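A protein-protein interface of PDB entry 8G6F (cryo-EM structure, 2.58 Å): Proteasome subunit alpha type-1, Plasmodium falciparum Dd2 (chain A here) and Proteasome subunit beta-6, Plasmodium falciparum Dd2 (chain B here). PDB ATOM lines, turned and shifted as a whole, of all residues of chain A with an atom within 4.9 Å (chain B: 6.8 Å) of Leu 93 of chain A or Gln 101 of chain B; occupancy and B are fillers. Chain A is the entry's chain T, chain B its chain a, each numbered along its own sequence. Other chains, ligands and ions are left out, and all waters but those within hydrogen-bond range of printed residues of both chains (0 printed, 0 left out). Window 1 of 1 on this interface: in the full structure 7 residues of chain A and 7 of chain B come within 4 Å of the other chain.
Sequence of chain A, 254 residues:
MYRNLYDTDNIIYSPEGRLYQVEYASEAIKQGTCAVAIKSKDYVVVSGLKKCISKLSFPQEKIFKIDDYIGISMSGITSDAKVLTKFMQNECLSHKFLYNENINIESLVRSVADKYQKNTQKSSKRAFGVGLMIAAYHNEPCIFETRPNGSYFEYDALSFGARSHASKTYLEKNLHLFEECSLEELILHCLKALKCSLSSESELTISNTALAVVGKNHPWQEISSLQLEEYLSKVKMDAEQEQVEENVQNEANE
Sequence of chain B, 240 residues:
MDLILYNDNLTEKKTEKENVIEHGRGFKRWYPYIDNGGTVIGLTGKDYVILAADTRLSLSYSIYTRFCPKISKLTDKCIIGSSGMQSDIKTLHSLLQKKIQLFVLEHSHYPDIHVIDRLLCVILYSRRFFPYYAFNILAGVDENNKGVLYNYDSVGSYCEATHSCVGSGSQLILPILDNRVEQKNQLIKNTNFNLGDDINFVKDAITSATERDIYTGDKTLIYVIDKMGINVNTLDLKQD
Gln 89 of chain A touches Leu 105 of chain B (NE2 to CD2, 3.7 Å).
Asn 90 of chain A touches Leu 102 of chain B.
Leu 93 of chain A touches Gln 101 of chain B.
Leu 93 of chain A touches Leu 102 of chain B.
CB of Ser 94 of chain A touches NZ of Lys 98 of chain B, at 3.9 Å.
O of Glu 91 of chain A lies within hydrogen-bond range of OG of Ser 94 of chain A (3.2 Å).
Of the printed residues of chain B, Gln 89 of chain A touches Leu 105 (3.7 Å).
Of the printed residues of chain B, Asn 90 of chain A touches Leu 102.
Of chain B, only Gln 101 and Leu 102 come within 4 Å of Leu 93 of chain A.
Of the printed residues of chain B, Ser 94 of chain A touches Lys 98 (3.9 Å).
Gln 101 of chain B touches just one residue of chain A: Leu 93 (3.4 Å).
Of the printed residues of chain A, Leu 102 of chain B touches Asn 90 and Leu 93.
The nearest printed residue of chain A that does not touch Lys 98 of chain B is Phe 97 of chain A (4.03 Å).
Hydrophobic or aromatic side chains of chain A within 4 Å of the printed part of chain B: Leu 93.
Printed residues of chain B that touch a printed residue of chain A: Lys 98, Gln 101, Leu 102 and Leu 105.
Hydrophobic or aromatic side chains of chain B within 4 Å of the printed part of chain A: Leu 102 and Leu 105.
Among the printed residues, no Asp or Glu carboxylate lies within 4 Å of a Lys or Arg side-chain nitrogen of the other chain.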
ATOM      1  N   GLN A  89      29.302  10.145  23.925  1.00  0.00           N
ATOM      2  CA  GLN A  89      27.850  10.022  23.906  1.00  0.00           C
ATOM      3  C   GLN A  89      27.430   8.566  23.773  1.00  0.00           C
ATOM      4  O   GLN A  89      26.531   8.101  24.486  1.00  0.00           O
ATOM      5  CB  GLN A  89      27.271  10.859  22.764  1.00  0.00           C
ATOM      6  CG  GLN A  89      27.326  12.352  23.020  1.00  0.00           C
ATOM      7  CD  GLN A  89      27.004  13.177  21.796  1.00  0.00           C
ATOM      8  OE1 GLN A  89      26.973  12.669  20.679  1.00  0.00           O
ATOM      9  NE2 GLN A  89      26.764  14.463  22.000  1.00  0.00           N
ATOM     10  N   ASN A  90      28.084   7.827  22.879  1.00  0.00           N
ATOM     11  CA  ASN A  90      27.748   6.420  22.717  1.00  0.00           C
ATOM     12  C   ASN A  90      28.083   5.624  23.968  1.00  0.00           C
ATOM     13  O   ASN A  90      27.347   4.706  24.333  1.00  0.00           O
ATOM     14  CB  ASN A  90      28.468   5.851  21.500  1.00  0.00           C
ATOM     15  CG  ASN A  90      27.773   6.199  20.205  1.00  0.00           C
ATOM     16  OD1 ASN A  90      26.673   5.723  19.932  1.00  0.00           O
ATOM     17  ND2 ASN A  90      28.404   7.042  19.403  1.00  0.00           N
ATOM     18  N   GLU A  91      29.185   5.956  24.641  1.00  0.00           N
ATOM     19  CA  GLU A  91      29.532   5.249  25.869  1.00  0.00           C
ATOM     20  C   GLU A  91      28.472   5.461  26.942  1.00  0.00           C
ATOM     21  O   GLU A  91      28.035   4.508  27.600  1.00  0.00           O
ATOM     22  CB  GLU A  91      30.899   5.710  26.368  1.00  0.00           C
ATOM     23  CG  GLU A  91      32.062   5.122  25.602  1.00  0.00           C
ATOM     24  CD  GLU A  91      32.143   3.617  25.731  1.00  0.00           C
ATOM     25  OE1 GLU A  91      32.492   3.130  26.825  1.00  0.00           O
ATOM     26  OE2 GLU A  91      31.851   2.917  24.741  1.00  0.00           O
ATOM     27  N   CYS A  92      28.041   6.707  27.131  1.00  0.00           N
ATOM     28  CA  CYS A  92      27.015   6.980  28.132  1.00  0.00           C
ATOM     29  C   CYS A  92      25.712   6.271  27.789  1.00  0.00           C
ATOM     30  O   CYS A  92      25.082   5.649  28.657  1.00  0.00           O
ATOM     31  CB  CYS A  92      26.789   8.485  28.250  1.00  0.00           C
ATOM     32  SG  CYS A  92      28.178   9.397  28.936  1.00  0.00           S
ATOM     33  N   LEU A  93      25.296   6.340  26.523  1.00  0.00           N
ATOM     34  CA  LEU A  93      24.044   5.710  26.127  1.00  0.00           C
ATOM     35  C   LEU A  93      24.114   4.197  26.271  1.00  0.00           C
ATOM     36  O   LEU A  93      23.147   3.569  26.712  1.00  0.00           O
ATOM     37  CB  LEU A  93      23.696   6.096  24.692  1.00  0.00           C
ATOM     38  CG  LEU A  93      23.146   7.510  24.521  1.00  0.00           C
ATOM     39  CD1 LEU A  93      23.218   7.931  23.072  1.00  0.00           C
ATOM     40  CD2 LEU A  93      21.728   7.600  25.036  1.00  0.00           C
ATOM     41  N   SER A  94      25.241   3.591  25.900  1.00  0.00           N
ATOM     42  CA  SER A  94      25.367   2.146  26.002  1.00  0.00           C
ATOM     43  C   SER A  94      25.414   1.690  27.451  1.00  0.00           C
ATOM     44  O   SER A  94      24.880   0.628  27.778  1.00  0.00           O
ATOM     45  CB  SER A  94      26.610   1.672  25.253  1.00  0.00           C
ATOM     46  OG  SER A  94      27.746   1.682  26.092  1.00  0.00           O
ATOM     47  N   HIS A  95      26.038   2.467  28.336  1.00  0.00           N
ATOM     48  CA  HIS A  95      25.975   2.125  29.750  1.00  0.00           C
ATOM     49  C   HIS A  95      24.544   2.188  30.262  1.00  0.00           C
ATOM     50  O   HIS A  95      24.103   1.303  31.004  1.00  0.00           O
ATOM     51  CB  HIS A  95      26.871   3.053  30.565  1.00  0.00           C
ATOM     52  CG  HIS A  95      27.099   2.582  31.966  1.00  0.00           C
ATOM     53  ND1 HIS A  95      28.187   1.820  32.324  1.00  0.00           N
ATOM     54  CD2 HIS A  95      26.370   2.752  33.093  1.00  0.00           C
ATOM     55  CE1 HIS A  95      28.126   1.549  33.615  1.00  0.00           C
ATOM     56  NE2 HIS A  95      27.033   2.103  34.104  1.00  0.00           N
ATOM     57  N   LYS A  96      23.800   3.226  29.878  1.00  0.00           N
ATOM     58  CA  LYS A  96      22.404   3.310  30.298  1.00  0.00           C
ATOM     59  C   LYS A  96      21.600   2.133  29.763  1.00  0.00           C
ATOM     60  O   LYS A  96      20.728   1.599  30.455  1.00  0.00           O
ATOM     61  CB  LYS A  96      21.794   4.629  29.831  1.00  0.00           C
ATOM     62  CG  LYS A  96      21.974   5.759  30.818  1.00  0.00           C
ATOM     63  CD  LYS A  96      21.443   7.069  30.278  1.00  0.00           C
ATOM     64  CE  LYS A  96      21.700   8.205  31.251  1.00  0.00           C
ATOM     65  NZ  LYS A  96      21.290   9.527  30.701  1.00  0.00           N
ATOM     66  N   PHE A  97      21.879   1.721  28.529  1.00  0.00           N
ATOM     67  CA  PHE A  97      21.178   0.590  27.935  1.00  0.00           C
ATOM     68  C   PHE A  97      21.489  -0.707  28.671  1.00  0.00           C
ATOM     69  O   PHE A  97      20.585  -1.496  28.970  1.00  0.00           O
ATOM     70  CB  PHE A  97      21.558   0.477  26.460  1.00  0.00           C
ATOM     71  CG  PHE A  97      21.126  -0.805  25.813  1.00  0.00           C
ATOM     72  CD1 PHE A  97      19.813  -0.992  25.427  1.00  0.00           C
ATOM     73  CD2 PHE A  97      22.038  -1.815  25.571  1.00  0.00           C
ATOM     74  CE1 PHE A  97      19.417  -2.163  24.825  1.00  0.00           C
ATOM     75  CE2 PHE A  97      21.645  -2.989  24.968  1.00  0.00           C
ATOM     76  CZ  PHE A  97      20.331  -3.162  24.595  1.00  0.00           C
ATOM     77  N   LYS B  73       7.780   5.028  28.147  1.00  0.00           N
ATOM     78  CA  LYS B  73       7.705   6.377  27.606  1.00  0.00           C
ATOM     79  C   LYS B  73       8.921   6.647  26.732  1.00  0.00           C
ATOM     80  O   LYS B  73      10.059   6.531  27.195  1.00  0.00           O
ATOM     81  CB  LYS B  73       7.627   7.396  28.744  1.00  0.00           C
ATOM     82  CG  LYS B  73       7.764   8.846  28.315  1.00  0.00           C
ATOM     83  CD  LYS B  73       7.881   9.763  29.511  1.00  0.00           C
ATOM     84  CE  LYS B  73       8.005  11.215  29.089  1.00  0.00           C
ATOM     85  NZ  LYS B  73       7.364  12.126  30.072  1.00  0.00           N
ATOM     86  N   LEU B  74       8.685   7.006  25.472  1.00  0.00           N
ATOM     87  CA  LEU B  74       9.765   7.280  24.535  1.00  0.00           C
ATOM     88  C   LEU B  74      10.077   8.763  24.424  1.00  0.00           C
ATOM     89  O   LEU B  74      11.247   9.150  24.437  1.00  0.00           O
ATOM     90  CB  LEU B  74       9.407   6.729  23.154  1.00  0.00           C
ATOM     91  CG  LEU B  74       8.991   5.260  23.131  1.00  0.00           C
ATOM     92  CD1 LEU B  74       8.454   4.885  21.772  1.00  0.00           C
ATOM     93  CD2 LEU B  74      10.161   4.374  23.512  1.00  0.00           C
ATOM     94  N   THR B  75       9.047   9.594  24.316  1.00  0.00           N
ATOM     95  CA  THR B  75       9.182  11.039  24.283  1.00  0.00           C
ATOM     96  C   THR B  75       8.054  11.618  25.122  1.00  0.00           C
ATOM     97  O   THR B  75       7.219  10.886  25.657  1.00  0.00           O
ATOM     98  CB  THR B  75       9.145  11.560  22.840  1.00  0.00           C
ATOM     99  OG1 THR B  75       9.907  10.692  21.996  1.00  0.00           O
ATOM    100  CG2 THR B  75       9.719  12.957  22.750  1.00  0.00           C
ATOM    101  N   LEU B  96      15.011   1.002  21.643  1.00  0.00           N
ATOM    102  CA  LEU B  96      14.317   2.137  21.052  1.00  0.00           C
ATOM    103  C   LEU B  96      14.621   3.421  21.810  1.00  0.00           C
ATOM    104  O   LEU B  96      14.839   4.473  21.200  1.00  0.00           O
ATOM    105  CB  LEU B  96      12.812   1.870  21.032  1.00  0.00           C
ATOM    106  CG  LEU B  96      11.943   2.711  20.097  1.00  0.00           C
ATOM    107  CD1 LEU B  96      12.521   2.775  18.698  1.00  0.00           C
ATOM    108  CD2 LEU B  96      10.537   2.161  20.071  1.00  0.00           C
ATOM    109  N   GLN B  97      14.630   3.361  23.142  1.00  0.00           N
ATOM    110  CA  GLN B  97      14.937   4.552  23.927  1.00  0.00           C
ATOM    111  C   GLN B  97      16.356   5.036  23.662  1.00  0.00           C
ATOM    112  O   GLN B  97      16.602   6.242  23.549  1.00  0.00           O
ATOM    113  CB  GLN B  97      14.736   4.262  25.411  1.00  0.00           C
ATOM    114  CG  GLN B  97      13.348   4.610  25.910  1.00  0.00           C
ATOM    115  CD  GLN B  97      12.951   3.833  27.142  1.00  0.00           C
ATOM    116  OE1 GLN B  97      13.654   2.921  27.572  1.00  0.00           O
ATOM    117  NE2 GLN B  97      11.813   4.187  27.718  1.00  0.00           N
ATOM    118  N   LYS B  98      17.305   4.105  23.565  1.00  0.00           N
ATOM    119  CA  LYS B  98      18.681   4.474  23.254  1.00  0.00           C
ATOM    120  C   LYS B  98      18.775   5.117  21.877  1.00  0.00           C
ATOM    121  O   LYS B  98      19.470   6.123  21.699  1.00  0.00           O
ATOM    122  CB  LYS B  98      19.570   3.234  23.339  1.00  0.00           C
ATOM    123  CG  LYS B  98      21.004   3.424  22.885  1.00  0.00           C
ATOM    124  CD  LYS B  98      21.707   2.089  22.768  1.00  0.00           C
ATOM    125  CE  LYS B  98      23.167   2.265  22.431  1.00  0.00           C
ATOM    126  NZ  LYS B  98      23.918   0.991  22.554  1.00  0.00           N
ATOM    127  N   LYS B  99      18.080   4.550  20.891  1.00  0.00           N
ATOM    128  CA  LYS B  99      18.094   5.121  19.550  1.00  0.00           C
ATOM    129  C   LYS B  99      17.502   6.520  19.543  1.00  0.00           C
ATOM    130  O   LYS B  99      18.004   7.410  18.851  1.00  0.00           O
ATOM    131  CB  LYS B  99      17.326   4.220  18.586  1.00  0.00           C
ATOM    132  CG  LYS B  99      18.007   2.905  18.296  1.00  0.00           C
ATOM    133  CD  LYS B  99      18.826   2.972  17.025  1.00  0.00           C
ATOM    134  CE  LYS B  99      19.870   1.875  16.994  1.00  0.00           C
ATOM    135  NZ  LYS B  99      19.278   0.532  17.238  1.00  0.00           N
ATOM    136  N   ILE B 100      16.429   6.736  20.301  1.00  0.00           N
ATOM    137  CA  ILE B 100      15.790   8.047  20.316  1.00  0.00           C
ATOM    138  C   ILE B 100      16.683   9.070  21.006  1.00  0.00           C
ATOM    139  O   ILE B 100      16.779  10.223  20.570  1.00  0.00           O
ATOM    140  CB  ILE B 100      14.407   7.958  20.981  1.00  0.00           C
ATOM    141  CG1 ILE B 100      13.435   7.213  20.071  1.00  0.00           C
ATOM    142  CG2 ILE B 100      13.868   9.340  21.282  1.00  0.00           C
ATOM    143  CD1 ILE B 100      12.228   6.677  20.788  1.00  0.00           C
ATOM    144  N   GLN B 101      17.345   8.679  22.094  1.00  0.00           N
ATOM    145  CA  GLN B 101      18.256   9.606  22.759  1.00  0.00           C
ATOM    146  C   GLN B 101      19.439   9.947  21.865  1.00  0.00           C
ATOM    147  O   GLN B 101      19.874  11.105  21.812  1.00  0.00           O
ATOM    148  CB  GLN B 101      18.741   9.013  24.080  1.00  0.00           C
ATOM    149  CG  GLN B 101      17.694   8.939  25.181  1.00  0.00           C
ATOM    150  CD  GLN B 101      16.714  10.091  25.156  1.00  0.00           C
ATOM    151  OE1 GLN B 101      17.081  11.238  25.406  1.00  0.00           O
ATOM    152  NE2 GLN B 101      15.457   9.792  24.853  1.00  0.00           N
ATOM    153  N   LEU B 102      19.975   8.956  21.154  1.00  0.00           N
ATOM    154  CA  LEU B 102      21.050   9.227  20.210  1.00  0.00           C
ATOM    155  C   LEU B 102      20.577  10.143  19.091  1.00  0.00           C
ATOM    156  O   LEU B 102      21.315  11.031  18.655  1.00  0.00           O
ATOM    157  CB  LEU B 102      21.583   7.913  19.645  1.00  0.00           C
ATOM    158  CG  LEU B 102      22.874   7.974  18.832  1.00  0.00           C
ATOM    159  CD1 LEU B 102      24.024   8.505  19.665  1.00  0.00           C
ATOM    160  CD2 LEU B 102      23.199   6.600  18.289  1.00  0.00           C
ATOM    161  N   PHE B 103      19.350   9.941  18.610  1.00  0.00           N
ATOM    162  CA  PHE B 103      18.792  10.830  17.599  1.00  0.00           C
ATOM    163  C   PHE B 103      18.698  12.254  18.120  1.00  0.00           C
ATOM    164  O   PHE B 103      19.039  13.206  17.413  1.00  0.00           O
ATOM    165  CB  PHE B 103      17.411  10.327  17.171  1.00  0.00           C
ATOM    166  CG  PHE B 103      16.783  11.129  16.065  1.00  0.00           C
ATOM    167  CD1 PHE B 103      16.138  12.319  16.334  1.00  0.00           C
ATOM    168  CD2 PHE B 103      16.828  10.683  14.760  1.00  0.00           C
ATOM    169  CE1 PHE B 103      15.565  13.050  15.325  1.00  0.00           C
ATOM    170  CE2 PHE B 103      16.253  11.415  13.748  1.00  0.00           C
ATOM    171  CZ  PHE B 103      15.620  12.595  14.032  1.00  0.00           C
ATOM    172  N   VAL B 104      18.230  12.422  19.353  1.00  0.00           N
ATOM    173  CA  VAL B 104      18.127  13.761  19.923  1.00  0.00           C
ATOM    174  C   VAL B 104      19.501  14.406  20.002  1.00  0.00           C
ATOM    175  O   VAL B 104      19.672  15.580  19.658  1.00  0.00           O
ATOM    176  CB  VAL B 104      17.454  13.703  21.305  1.00  0.00           C
ATOM    177  CG1 VAL B 104      17.525  15.054  21.976  1.00  0.00           C
ATOM    178  CG2 VAL B 104      16.015  13.247  21.178  1.00  0.00           C
ATOM    179  N   LEU B 105      20.501  13.653  20.459  1.00  0.00           N
ATOM    180  CA  LEU B 105      21.839  14.222  20.586  1.00  0.00           C
ATOM    181  C   LEU B 105      22.415  14.596  19.227  1.00  0.00           C
ATOM    182  O   LEU B 105      23.072  15.633  19.089  1.00  0.00           O
ATOM    183  CB  LEU B 105      22.762  13.237  21.300  1.00  0.00           C
ATOM    184  CG  LEU B 105      22.738  13.291  22.826  1.00  0.00           C
ATOM    185  CD1 LEU B 105      23.528  12.133  23.391  1.00  0.00           C
ATOM    186  CD2 LEU B 105      23.276  14.615  23.340  1.00  0.00           C
ATOM    187  N   GLU B 106      22.182  13.764  18.214  1.00  0.00           N
ATOM    188  CA  GLU B 106      22.806  13.976  16.914  1.00  0.00           C
ATOM    189  C   GLU B 106      22.103  15.066  16.115  1.00  0.00           C
ATOM    190  O   GLU B 106      22.740  16.024  15.668  1.00  0.00           O
ATOM    191  CB  GLU B 106      22.813  12.667  16.128  1.00  0.00           C
ATOM    192  CG  GLU B 106      23.866  12.606  15.048  1.00  0.00           C
ATOM    193  CD  GLU B 106      24.014  11.221  14.463  1.00  0.00           C
ATOM    194  OE1 GLU B 106      23.354  10.290  14.970  1.00  0.00           O
ATOM    195  OE2 GLU B 106      24.791  11.061  13.498  1.00  0.00           O
ATOM    196  N   TYR B 110      13.681  16.229  18.926  1.00  0.00           N
ATOM    197  CA  TYR B 110      13.032  14.975  19.294  1.00  0.00           C
ATOM    198  C   TYR B 110      12.251  14.421  18.109  1.00  0.00           C
ATOM    199  O   TYR B 110      11.477  15.156  17.490  1.00  0.00           O
ATOM    200  CB  TYR B 110      12.096  15.173  20.478  1.00  0.00           C
ATOM    201  CG  TYR B 110      12.816  15.186  21.799  1.00  0.00           C
ATOM    202  CD1 TYR B 110      13.320  16.366  22.321  1.00  0.00           C
ATOM    203  CD2 TYR B 110      13.012  14.015  22.516  1.00  0.00           C
ATOM    204  CE1 TYR B 110      13.988  16.383  23.522  1.00  0.00           C
ATOM    205  CE2 TYR B 110      13.678  14.022  23.720  1.00  0.00           C
ATOM    206  CZ  TYR B 110      14.167  15.210  24.218  1.00  0.00           C
ATOM    207  OH  TYR B 110      14.836  15.230  25.418  1.00  0.00           O
ATOM    208  N   PRO B 111      12.418  13.146  17.768  1.00  0.00           N
ATOM    209  CA  PRO B 111      11.618  12.579  16.684  1.00  0.00           C
ATOM    210  C   PRO B 111      10.154  12.503  17.075  1.00  0.00           C
ATOM    211  O   PRO B 111       9.808  12.335  18.245  1.00  0.00           O
ATOM    212  CB  PRO B 111      12.222  11.185  16.492  1.00  0.00           C
ATOM    213  CG  PRO B 111      12.767  10.841  17.818  1.00  0.00           C
ATOM    214  CD  PRO B 111      13.244  12.120  18.428  1.00  0.00           C
